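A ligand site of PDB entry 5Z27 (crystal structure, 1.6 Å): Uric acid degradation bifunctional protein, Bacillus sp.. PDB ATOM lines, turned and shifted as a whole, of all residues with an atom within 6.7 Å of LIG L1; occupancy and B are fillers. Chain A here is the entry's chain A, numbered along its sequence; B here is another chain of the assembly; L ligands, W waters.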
ATOM      1  N   SER A 182      -4.777  24.782  -9.898  1.00  0.00           N
ATOM      2  CA  SER A 182      -4.083  24.350  -8.698  1.00  0.00           C
ATOM      3  C   SER A 182      -4.586  25.125  -7.487  1.00  0.00           C
ATOM      4  O   SER A 182      -5.123  26.234  -7.598  1.00  0.00           O
ATOM      5  CB  SER A 182      -2.570  24.524  -8.826  1.00  0.00           C
ATOM      6  OG  SER A 182      -2.198  25.861  -8.558  1.00  0.00           O
ATOM      7  N   PHE A 183      -4.409  24.521  -6.324  1.00  0.00           N
ATOM      8  CA  PHE A 183      -4.536  25.263  -5.068  1.00  0.00           C
ATOM      9  C   PHE A 183      -3.462  24.702  -4.145  1.00  0.00           C
ATOM     10  O   PHE A 183      -3.640  23.651  -3.538  1.00  0.00           O
ATOM     11  CB  PHE A 183      -5.919  25.129  -4.454  1.00  0.00           C
ATOM     12  CG  PHE A 183      -6.135  26.032  -3.278  1.00  0.00           C
ATOM     13  CD1 PHE A 183      -6.005  27.410  -3.423  1.00  0.00           C
ATOM     14  CD2 PHE A 183      -6.434  25.529  -2.018  1.00  0.00           C
ATOM     15  CE1 PHE A 183      -6.177  28.260  -2.344  1.00  0.00           C
ATOM     16  CE2 PHE A 183      -6.606  26.379  -0.939  1.00  0.00           C
ATOM     17  CZ  PHE A 183      -6.476  27.753  -1.106  1.00  0.00           C
ATOM     18  N   PHE A 186      -1.077  27.226   0.653  1.00  0.00           N
ATOM     19  CA  PHE A 186      -1.867  27.813   1.721  1.00  0.00           C
ATOM     20  C   PHE A 186      -1.328  27.372   3.086  1.00  0.00           C
ATOM     21  O   PHE A 186      -0.471  26.475   3.195  1.00  0.00           O
ATOM     22  CB  PHE A 186      -3.349  27.455   1.569  1.00  0.00           C
ATOM     23  CG  PHE A 186      -3.611  25.973   1.370  1.00  0.00           C
ATOM     24  CD1 PHE A 186      -3.590  25.421   0.095  1.00  0.00           C
ATOM     25  CD2 PHE A 186      -3.845  25.149   2.457  1.00  0.00           C
ATOM     26  CE1 PHE A 186      -3.811  24.081  -0.092  1.00  0.00           C
ATOM     27  CE2 PHE A 186      -4.072  23.802   2.266  1.00  0.00           C
ATOM     28  CZ  PHE A 186      -4.051  23.264   0.992  1.00  0.00           C
ATOM     29  N   LEU A 194      -6.731  19.813   4.439  1.00  0.00           N
ATOM     30  CA  LEU A 194      -6.864  19.858   2.980  1.00  0.00           C
ATOM     31  C   LEU A 194      -5.542  19.558   2.281  1.00  0.00           C
ATOM     32  O   LEU A 194      -4.567  20.275   2.494  1.00  0.00           O
ATOM     33  CB  LEU A 194      -7.379  21.229   2.541  1.00  0.00           C
ATOM     34  CG  LEU A 194      -7.584  21.453   1.053  1.00  0.00           C
ATOM     35  CD1 LEU A 194      -8.805  20.691   0.556  1.00  0.00           C
ATOM     36  CD2 LEU A 194      -7.743  22.945   0.734  1.00  0.00           C
ATOM     37  N   ARG A 200      -6.869  20.274  -9.885  1.00  0.00           N
ATOM     38  CA  ARG A 200      -8.226  20.009  -9.438  1.00  0.00           C
ATOM     39  C   ARG A 200      -9.227  20.417 -10.511  1.00  0.00           C
ATOM     40  O   ARG A 200      -8.955  21.326 -11.303  1.00  0.00           O
ATOM     41  CB  ARG A 200      -8.544  20.769  -8.157  1.00  0.00           C
ATOM     42  CG  ARG A 200      -8.425  22.267  -8.292  1.00  0.00           C
ATOM     43  CD  ARG A 200      -8.721  22.941  -6.991  1.00  0.00           C
ATOM     44  NE  ARG A 200      -8.655  24.392  -7.109  1.00  0.00           N
ATOM     45  CZ  ARG A 200      -9.052  25.242  -6.171  1.00  0.00           C
ATOM     46  NH1 ARG A 200      -9.532  24.759  -5.033  1.00  0.00           N
ATOM     47  NH2 ARG A 200      -8.955  26.546  -6.370  1.00  0.00           N
ATOM     48  N   LEU A 202     -11.770  22.509 -10.853  1.00  0.00           N
ATOM     49  CA  LEU A 202     -12.380  23.631 -10.149  1.00  0.00           C
ATOM     50  C   LEU A 202     -13.777  23.912 -10.669  1.00  0.00           C
ATOM     51  O   LEU A 202     -13.981  24.127 -11.866  1.00  0.00           O
ATOM     52  CB  LEU A 202     -11.497  24.859 -10.301  1.00  0.00           C
ATOM     53  CG  LEU A 202     -12.032  26.143  -9.690  1.00  0.00           C
ATOM     54  CD1 LEU A 202     -12.229  25.955  -8.203  1.00  0.00           C
ATOM     55  CD2 LEU A 202     -11.067  27.280  -9.961  1.00  0.00           C
ATOM     56  N   LEU A 246      -4.836  29.540  -9.917  1.00  0.00           N
ATOM     57  CA  LEU A 246      -4.103  29.312  -8.678  1.00  0.00           C
ATOM     58  C   LEU A 246      -4.981  29.388  -7.445  1.00  0.00           C
ATOM     59  O   LEU A 246      -4.508  29.085  -6.337  1.00  0.00           O
ATOM     60  CB  LEU A 246      -2.969  30.334  -8.541  1.00  0.00           C
ATOM     61  CG  LEU A 246      -1.955  30.325  -9.692  1.00  0.00           C
ATOM     62  CD1 LEU A 246      -1.046  31.538  -9.619  1.00  0.00           C
ATOM     63  CD2 LEU A 246      -1.142  29.031  -9.690  1.00  0.00           C
ATOM     64  N   SER A 247      -6.246  29.773  -7.620  1.00  0.00           N
ATOM     65  CA  SER A 247      -7.264  29.930  -6.594  1.00  0.00           C
ATOM     66  C   SER A 247      -8.482  30.550  -7.241  1.00  0.00           C
ATOM     67  O   SER A 247      -8.367  31.129  -8.338  1.00  0.00           O
ATOM     68  CB  SER A 247      -6.792  30.826  -5.455  1.00  0.00           C
ATOM     69  OG  SER A 247      -6.583  32.150  -5.942  1.00  0.00           O
ATOM     70  N   ILE A 248      -9.635  30.506  -6.593  1.00  0.00           N
ATOM     71  CA  ILE A 248     -10.778  31.250  -7.100  1.00  0.00           C
ATOM     72  C   ILE A 248     -10.515  32.746  -6.964  1.00  0.00           C
ATOM     73  O   ILE A 248     -10.893  33.526  -7.839  1.00  0.00           O
ATOM     74  CB  ILE A 248     -12.078  30.839  -6.389  1.00  0.00           C
ATOM     75  CG1 ILE A 248     -12.409  29.392  -6.685  1.00  0.00           C
ATOM     76  CG2 ILE A 248     -13.227  31.728  -6.860  1.00  0.00           C
ATOM     77  CD1 ILE A 248     -13.455  28.837  -5.731  1.00  0.00           C
ATOM     78  N   GLN A 249      -9.861  33.155  -5.865  1.00  0.00           N
ATOM     79  CA  GLN A 249      -9.497  34.555  -5.658  1.00  0.00           C
ATOM     80  C   GLN A 249      -8.771  35.131  -6.863  1.00  0.00           C
ATOM     81  O   GLN A 249      -9.082  36.236  -7.340  1.00  0.00           O
ATOM     82  CB  GLN A 249      -8.591  34.666  -4.410  1.00  0.00           C
ATOM     83  CG  GLN A 249      -9.293  34.423  -3.049  1.00  0.00           C
ATOM     84  CD  GLN A 249      -9.316  32.969  -2.612  1.00  0.00           C
ATOM     85  OE1 GLN A 249      -9.551  32.053  -3.403  1.00  0.00           O
ATOM     86  NE2 GLN A 249      -9.105  32.744  -1.316  1.00  0.00           N
ATOM     87  N   ASN A 275     -17.179  28.013  -4.206  1.00  0.00           N
ATOM     88  CA  ASN A 275     -16.431  26.827  -4.583  1.00  0.00           C
ATOM     89  C   ASN A 275     -17.305  25.598  -4.352  1.00  0.00           C
ATOM     90  O   ASN A 275     -17.730  25.353  -3.219  1.00  0.00           O
ATOM     91  CB  ASN A 275     -15.145  26.726  -3.773  1.00  0.00           C
ATOM     92  CG  ASN A 275     -14.187  25.691  -4.299  1.00  0.00           C
ATOM     93  OD1 ASN A 275     -14.575  24.775  -5.009  1.00  0.00           O
ATOM     94  ND2 ASN A 275     -12.928  25.818  -3.926  1.00  0.00           N
ATOM     95  N   GLY A 301     -16.863  27.025  -0.013  1.00  0.00           N
ATOM     96  CA  GLY A 301     -16.088  28.253   0.074  1.00  0.00           C
ATOM     97  C   GLY A 301     -16.723  29.367  -0.743  1.00  0.00           C
ATOM     98  O   GLY A 301     -17.491  29.144  -1.681  1.00  0.00           O
ATOM     99  N   PHE A 302     -16.408  30.606  -0.369  1.00  0.00           N
ATOM    100  CA  PHE A 302     -16.912  31.733  -1.134  1.00  0.00           C
ATOM    101  C   PHE A 302     -15.926  32.889  -1.028  1.00  0.00           C
ATOM    102  O   PHE A 302     -15.074  32.941  -0.131  1.00  0.00           O
ATOM    103  CB  PHE A 302     -18.315  32.153  -0.658  1.00  0.00           C
ATOM    104  CG  PHE A 302     -18.379  32.668   0.747  1.00  0.00           C
ATOM    105  CD1 PHE A 302     -18.047  33.983   1.018  1.00  0.00           C
ATOM    106  CD2 PHE A 302     -18.798  31.850   1.784  1.00  0.00           C
ATOM    107  CE1 PHE A 302     -18.123  34.472   2.319  1.00  0.00           C
ATOM    108  CE2 PHE A 302     -18.868  32.333   3.086  1.00  0.00           C
ATOM    109  CZ  PHE A 302     -18.525  33.641   3.350  1.00  0.00           C
ATOM    110  N   GLN A 303     -16.038  33.788  -2.002  1.00  0.00           N
ATOM    111  CA  GLN A 303     -15.165  34.948  -2.111  1.00  0.00           C
ATOM    112  C   GLN A 303     -15.999  36.142  -2.532  1.00  0.00           C
ATOM    113  O   GLN A 303     -16.931  35.997  -3.320  1.00  0.00           O
ATOM    114  CB  GLN A 303     -14.045  34.722  -3.128  1.00  0.00           C
ATOM    115  CG  GLN A 303     -13.093  33.582  -2.838  1.00  0.00           C
ATOM    116  CD  GLN A 303     -13.649  32.180  -3.098  1.00  0.00           C
ATOM    117  OE1 GLN A 303     -14.632  31.991  -3.813  1.00  0.00           O
ATOM    118  NE2 GLN A 303     -12.991  31.184  -2.517  1.00  0.00           N
ATOM    119  N   TYR B  10     -13.439  36.445   2.065  1.00  0.00           N
ATOM    120  CA  TYR B  10     -13.631  35.049   1.666  1.00  0.00           C
ATOM    121  C   TYR B  10     -13.926  34.221   2.911  1.00  0.00           C
ATOM    122  O   TYR B  10     -13.668  34.649   4.032  1.00  0.00           O
ATOM    123  CB  TYR B  10     -12.411  34.503   0.899  1.00  0.00           C
ATOM    124  CG  TYR B  10     -11.258  34.030   1.754  1.00  0.00           C
ATOM    125  CD1 TYR B  10     -10.530  34.923   2.528  1.00  0.00           C
ATOM    126  CD2 TYR B  10     -10.891  32.690   1.772  1.00  0.00           C
ATOM    127  CE1 TYR B  10      -9.476  34.490   3.306  1.00  0.00           C
ATOM    128  CE2 TYR B  10      -9.829  32.245   2.531  1.00  0.00           C
ATOM    129  CZ  TYR B  10      -9.135  33.150   3.314  1.00  0.00           C
ATOM    130  OH  TYR B  10      -8.098  32.730   4.098  1.00  0.00           O
ATOM    131  N   GLY B  11     -14.485  33.042   2.698  1.00  0.00           N
ATOM    132  CA  GLY B  11     -14.945  32.268   3.842  1.00  0.00           C
ATOM    133  C   GLY B  11     -15.636  30.988   3.458  1.00  0.00           C
ATOM    134  O   GLY B  11     -15.427  30.453   2.366  1.00  0.00           O
ATOM    135  N   LYS B  12     -16.452  30.493   4.390  1.00  0.00           N
ATOM    136  CA  LYS B  12     -17.100  29.204   4.248  1.00  0.00           C
ATOM    137  C   LYS B  12     -18.536  29.319   4.708  1.00  0.00           C
ATOM    138  O   LYS B  12     -18.788  29.890   5.777  1.00  0.00           O
ATOM    139  CB  LYS B  12     -16.376  28.136   5.072  1.00  0.00           C
ATOM    140  CG  LYS B  12     -16.639  26.691   4.640  1.00  0.00           C
ATOM    141  CD  LYS B  12     -15.783  26.356   3.423  1.00  0.00           C
ATOM    142  CE  LYS B  12     -15.797  24.900   3.053  1.00  0.00           C
ATOM    143  NZ  LYS B  12     -14.735  24.593   2.048  1.00  0.00           N
ATOM    144  N   ASN B  66      -0.822  32.151  -2.137  1.00  0.00           N
ATOM    145  CA  ASN B  66      -1.660  31.647  -1.053  1.00  0.00           C
ATOM    146  C   ASN B  66      -0.942  31.586   0.285  1.00  0.00           C
ATOM    147  O   ASN B  66      -1.502  31.067   1.259  1.00  0.00           O
ATOM    148  CB  ASN B  66      -2.186  30.259  -1.430  1.00  0.00           C
ATOM    149  CG  ASN B  66      -3.160  30.315  -2.598  1.00  0.00           C
ATOM    150  OD1 ASN B  66      -4.044  31.176  -2.635  1.00  0.00           O
ATOM    151  ND2 ASN B  66      -2.987  29.424  -3.563  1.00  0.00           N
ATOM    152  N   VAL B  69      -3.139  32.548   3.096  1.00  0.00           N
ATOM    153  CA  VAL B  69      -4.526  32.083   2.990  1.00  0.00           C
ATOM    154  C   VAL B  69      -4.750  30.962   3.991  1.00  0.00           C
ATOM    155  O   VAL B  69      -4.109  29.905   3.911  1.00  0.00           O
ATOM    156  CB  VAL B  69      -4.853  31.620   1.558  1.00  0.00           C
ATOM    157  CG1 VAL B  69      -6.238  30.980   1.487  1.00  0.00           C
ATOM    158  CG2 VAL B  69      -4.761  32.781   0.607  1.00  0.00           C
ATOM    159  N   VAL B  70      -5.645  31.203   4.935  1.00  0.00           N
ATOM    160  CA  VAL B  70      -6.267  30.114   5.689  1.00  0.00           C
ATOM    161  C   VAL B  70      -7.260  29.448   4.763  1.00  0.00           C
ATOM    162  O   VAL B  70      -8.222  30.086   4.314  1.00  0.00           O
ATOM    163  CB  VAL B  70      -6.957  30.650   6.951  1.00  0.00           C
ATOM    164  CG1 VAL B  70      -7.638  29.508   7.720  1.00  0.00           C
ATOM    165  CG2 VAL B  70      -5.974  31.378   7.827  1.00  0.00           C
ATOM    166  N   ALA B  71      -7.036  28.180   4.444  1.00  0.00           N
ATOM    167  CA  ALA B  71      -7.980  27.466   3.585  1.00  0.00           C
ATOM    168  C   ALA B  71      -9.384  27.504   4.178  1.00  0.00           C
ATOM    169  O   ALA B  71      -9.570  27.443   5.404  1.00  0.00           O
ATOM    170  CB  ALA B  71      -7.549  26.016   3.378  1.00  0.00           C
ATOM    171  N   THR B  72     -10.387  27.656   3.322  1.00  0.00           N
ATOM    172  CA  THR B  72     -11.749  27.688   3.845  1.00  0.00           C
ATOM    173  C   THR B  72     -12.115  26.360   4.465  1.00  0.00           C
ATOM    174  O   THR B  72     -12.885  26.318   5.435  1.00  0.00           O
ATOM    175  CB  THR B  72     -12.742  28.071   2.750  1.00  0.00           C
ATOM    176  OG1 THR B  72     -12.794  27.016   1.777  1.00  0.00           O
ATOM    177  CG2 THR B  72     -12.347  29.385   2.075  1.00  0.00           C
ATOM    178  N   ASP B  73     -11.556  25.266   3.950  1.00  0.00           N
ATOM    179  CA  ASP B  73     -11.714  23.963   4.601  1.00  0.00           C
ATOM    180  C   ASP B  73     -11.182  23.999   6.029  1.00  0.00           C
ATOM    181  O   ASP B  73     -11.761  23.388   6.932  1.00  0.00           O
ATOM    182  CB  ASP B  73     -10.996  22.900   3.773  1.00  0.00           C
ATOM    183  CG  ASP B  73     -11.261  21.506   4.306  1.00  0.00           C
ATOM    184  OD1 ASP B  73     -12.334  20.951   3.999  1.00  0.00           O
ATOM    185  OD2 ASP B  73     -10.402  20.971   5.041  1.00  0.00           O
ATOM    186  N   SER B  74     -10.085  24.713   6.257  1.00  0.00           N
ATOM    187  CA  SER B  74      -9.547  24.835   7.612  1.00  0.00           C
ATOM    188  C   SER B  74     -10.437  25.678   8.509  1.00  0.00           C
ATOM    189  O   SER B  74     -10.522  25.424   9.708  1.00  0.00           O
ATOM    190  CB  SER B  74      -8.139  25.418   7.545  1.00  0.00           C
ATOM    191  OG  SER B  74      -7.336  24.631   6.697  1.00  0.00           O
ATOM    192  N   MET B  75     -11.110  26.693   7.946  1.00  0.00           N
ATOM    193  CA  MET B  75     -12.089  27.432   8.721  1.00  0.00           C
ATOM    194  C   MET B  75     -13.227  26.513   9.166  1.00  0.00           C
ATOM    195  O   MET B  75     -13.706  26.614  10.308  1.00  0.00           O
ATOM    196  CB  MET B  75     -12.651  28.585   7.893  1.00  0.00           C
ATOM    197  CG  MET B  75     -11.626  29.601   7.427  1.00  0.00           C
ATOM    198  SD  MET B  75     -12.455  30.828   6.408  1.00  0.00           S
ATOM    199  CE  MET B  75     -11.029  31.692   5.766  1.00  0.00           C
HETATM  200  N1  LIG L   1      -9.605  29.328  -2.447  1.00  0.00           N
HETATM  201  C1  LIG L   1      -9.664  28.325  -3.363  1.00  0.00           C
HETATM  202  O1  LIG L   1      -9.647  28.594  -4.523  1.00  0.00           O
HETATM  203  N2  LIG L   1      -9.770  27.060  -2.926  1.00  0.00           N
HETATM  204  C2  LIG L   1      -9.814  26.775  -1.617  1.00  0.00           C
HETATM  205  C3  LIG L   1      -9.735  27.780  -0.715  1.00  0.00           C
HETATM  206  C4  LIG L   1      -9.631  29.073  -1.149  1.00  0.00           C
HETATM  207  O2  LIG L   1      -9.585  29.999  -0.376  1.00  0.00           O
HETATM  208  N3  LIG L   1      -9.792  27.233   0.505  1.00  0.00           N
HETATM  209  N4  LIG L   1      -9.901  25.891   0.382  1.00  0.00           N
HETATM  210  N5  LIG L   1      -9.897  25.607  -0.944  1.00  0.00           N
HETATM  211  O1  LG2 L   2     -12.927  28.359  -2.002  1.00  0.00           O
HETATM  212  O2  LG2 L   2     -12.943  27.651  -1.066  1.00  0.00           O
HETATM  213  O   HOH W   1     -12.190  24.150   0.814  1.00  0.00           O
HETATM  214  O   HOH W   2     -10.262  23.102  -2.024  1.00  0.00           O
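Water W1 lies within hydrogen-bond range of the side-chain amino group (NZ) of Lys 12 of chain B (2.9 Å), a nitrogen (N4) of LIG L1 (2.9 Å), the side-chain hydroxyl (OG1) of Thr 72 of chain B (3.1 Å) and the backbone NH (N) of Asp 73 of chain B (3.4 Å).
Phe 183 touches LIG L1 (CZ to C3, 3.3 Å).
Leu 194 touches LIG L1 (CD2 to N4, 3.7 Å).
CA of Ser 247 touches O1 of LIG L1 (3.4 Å).
Asn 275 touches LIG L1 (ND2 to N2, 3.5 Å).
Gln 303 touches LIG L1 (NE2 to N1, 3.9 Å).
Tyr 10 of chain B touches LIG L1 (CE2 to O2, 3.7 Å).
Val 69 of chain B touches LIG L1 (CG1 to O2, 3.95 Å).
Ala 71 of chain B touches LIG L1.
Asp 73 of chain B touches LIG L1 (N to N4, 3.98 Å).
Hydrophobic or aromatic side chains within 4 Å of LIG L1: Phe 183, Leu 194, Ile 248, Tyr 10 of chain B, Val 69 of chain B and Ala 71 of chain B.
13 residues have an atom within 4 Å of LIG L1: Phe 183, Leu 194, Arg 200, Ser 247, Ile 248, Gln 249, Asn 275, Gln 303, Tyr 10 of chain B, Val 69 of chain B, Ala 71 of chain B, Thr 72 of chain B and Asp 73 of chain B.
The backbone NH (N) of Gln 249 lies close to the side-chain hydroxyl (OG) of Ser 247, 3.4 Å away.
The side-chain hydroxyl (OG1) of Thr 72 of chain B lies within hydrogen-bond range of the side-chain amino group (NZ) of Lys 12 of chain B, at 3.1 Å.
N of Asn 275 sits at hydrogen-bond distance from O of Gly 301, at 2.8 Å.
The backbone carbonyl oxygen (O) of Val 70 of chain B lies within hydrogen-bond range of the side-chain hydroxyl (OH) of Tyr 10 of chain B, 2.7 Å away.
An oxygen (O1) of LIG L1 sits at hydrogen-bond distance from the backbone NH (N) of Ile 248 (2.8 Å).
The guanidinium group of Arg 200 sits at hydrogen-bond distance from an oxygen (O1) of LIG L1, at 2.8 Å.
A nitrogen (N1) of LIG L1 lies within hydrogen-bond range of the side-chain amide oxygen (OE1) of Gln 249 (2.9 Å).
The backbone NH (N) of Thr 72 of chain B is in hydrogen-bond range of a nitrogen (N3) of LIG L1 (2.9 Å).
OG1 of Thr 72 of chain B is in hydrogen-bond range of N3 of LIG L1, at 3.3 Å.
An oxygen (O2) of LG2 L2 lies within hydrogen-bond range of the side-chain hydroxyl (OG1) of Thr 72 of chain B, 2.9 Å away.
An oxygen (O1) of LG2 L2 is in hydrogen-bond range of the side-chain amide nitrogen (ND2) of Asn 275, at 3.2 Å.
NE2 of Gln 303 lies within hydrogen-bond range of O1 of LG2 L2 (2.9 Å).
A nitrogen (N1) of LIG L1 lies close to an oxygen (O1) of LG2 L2.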
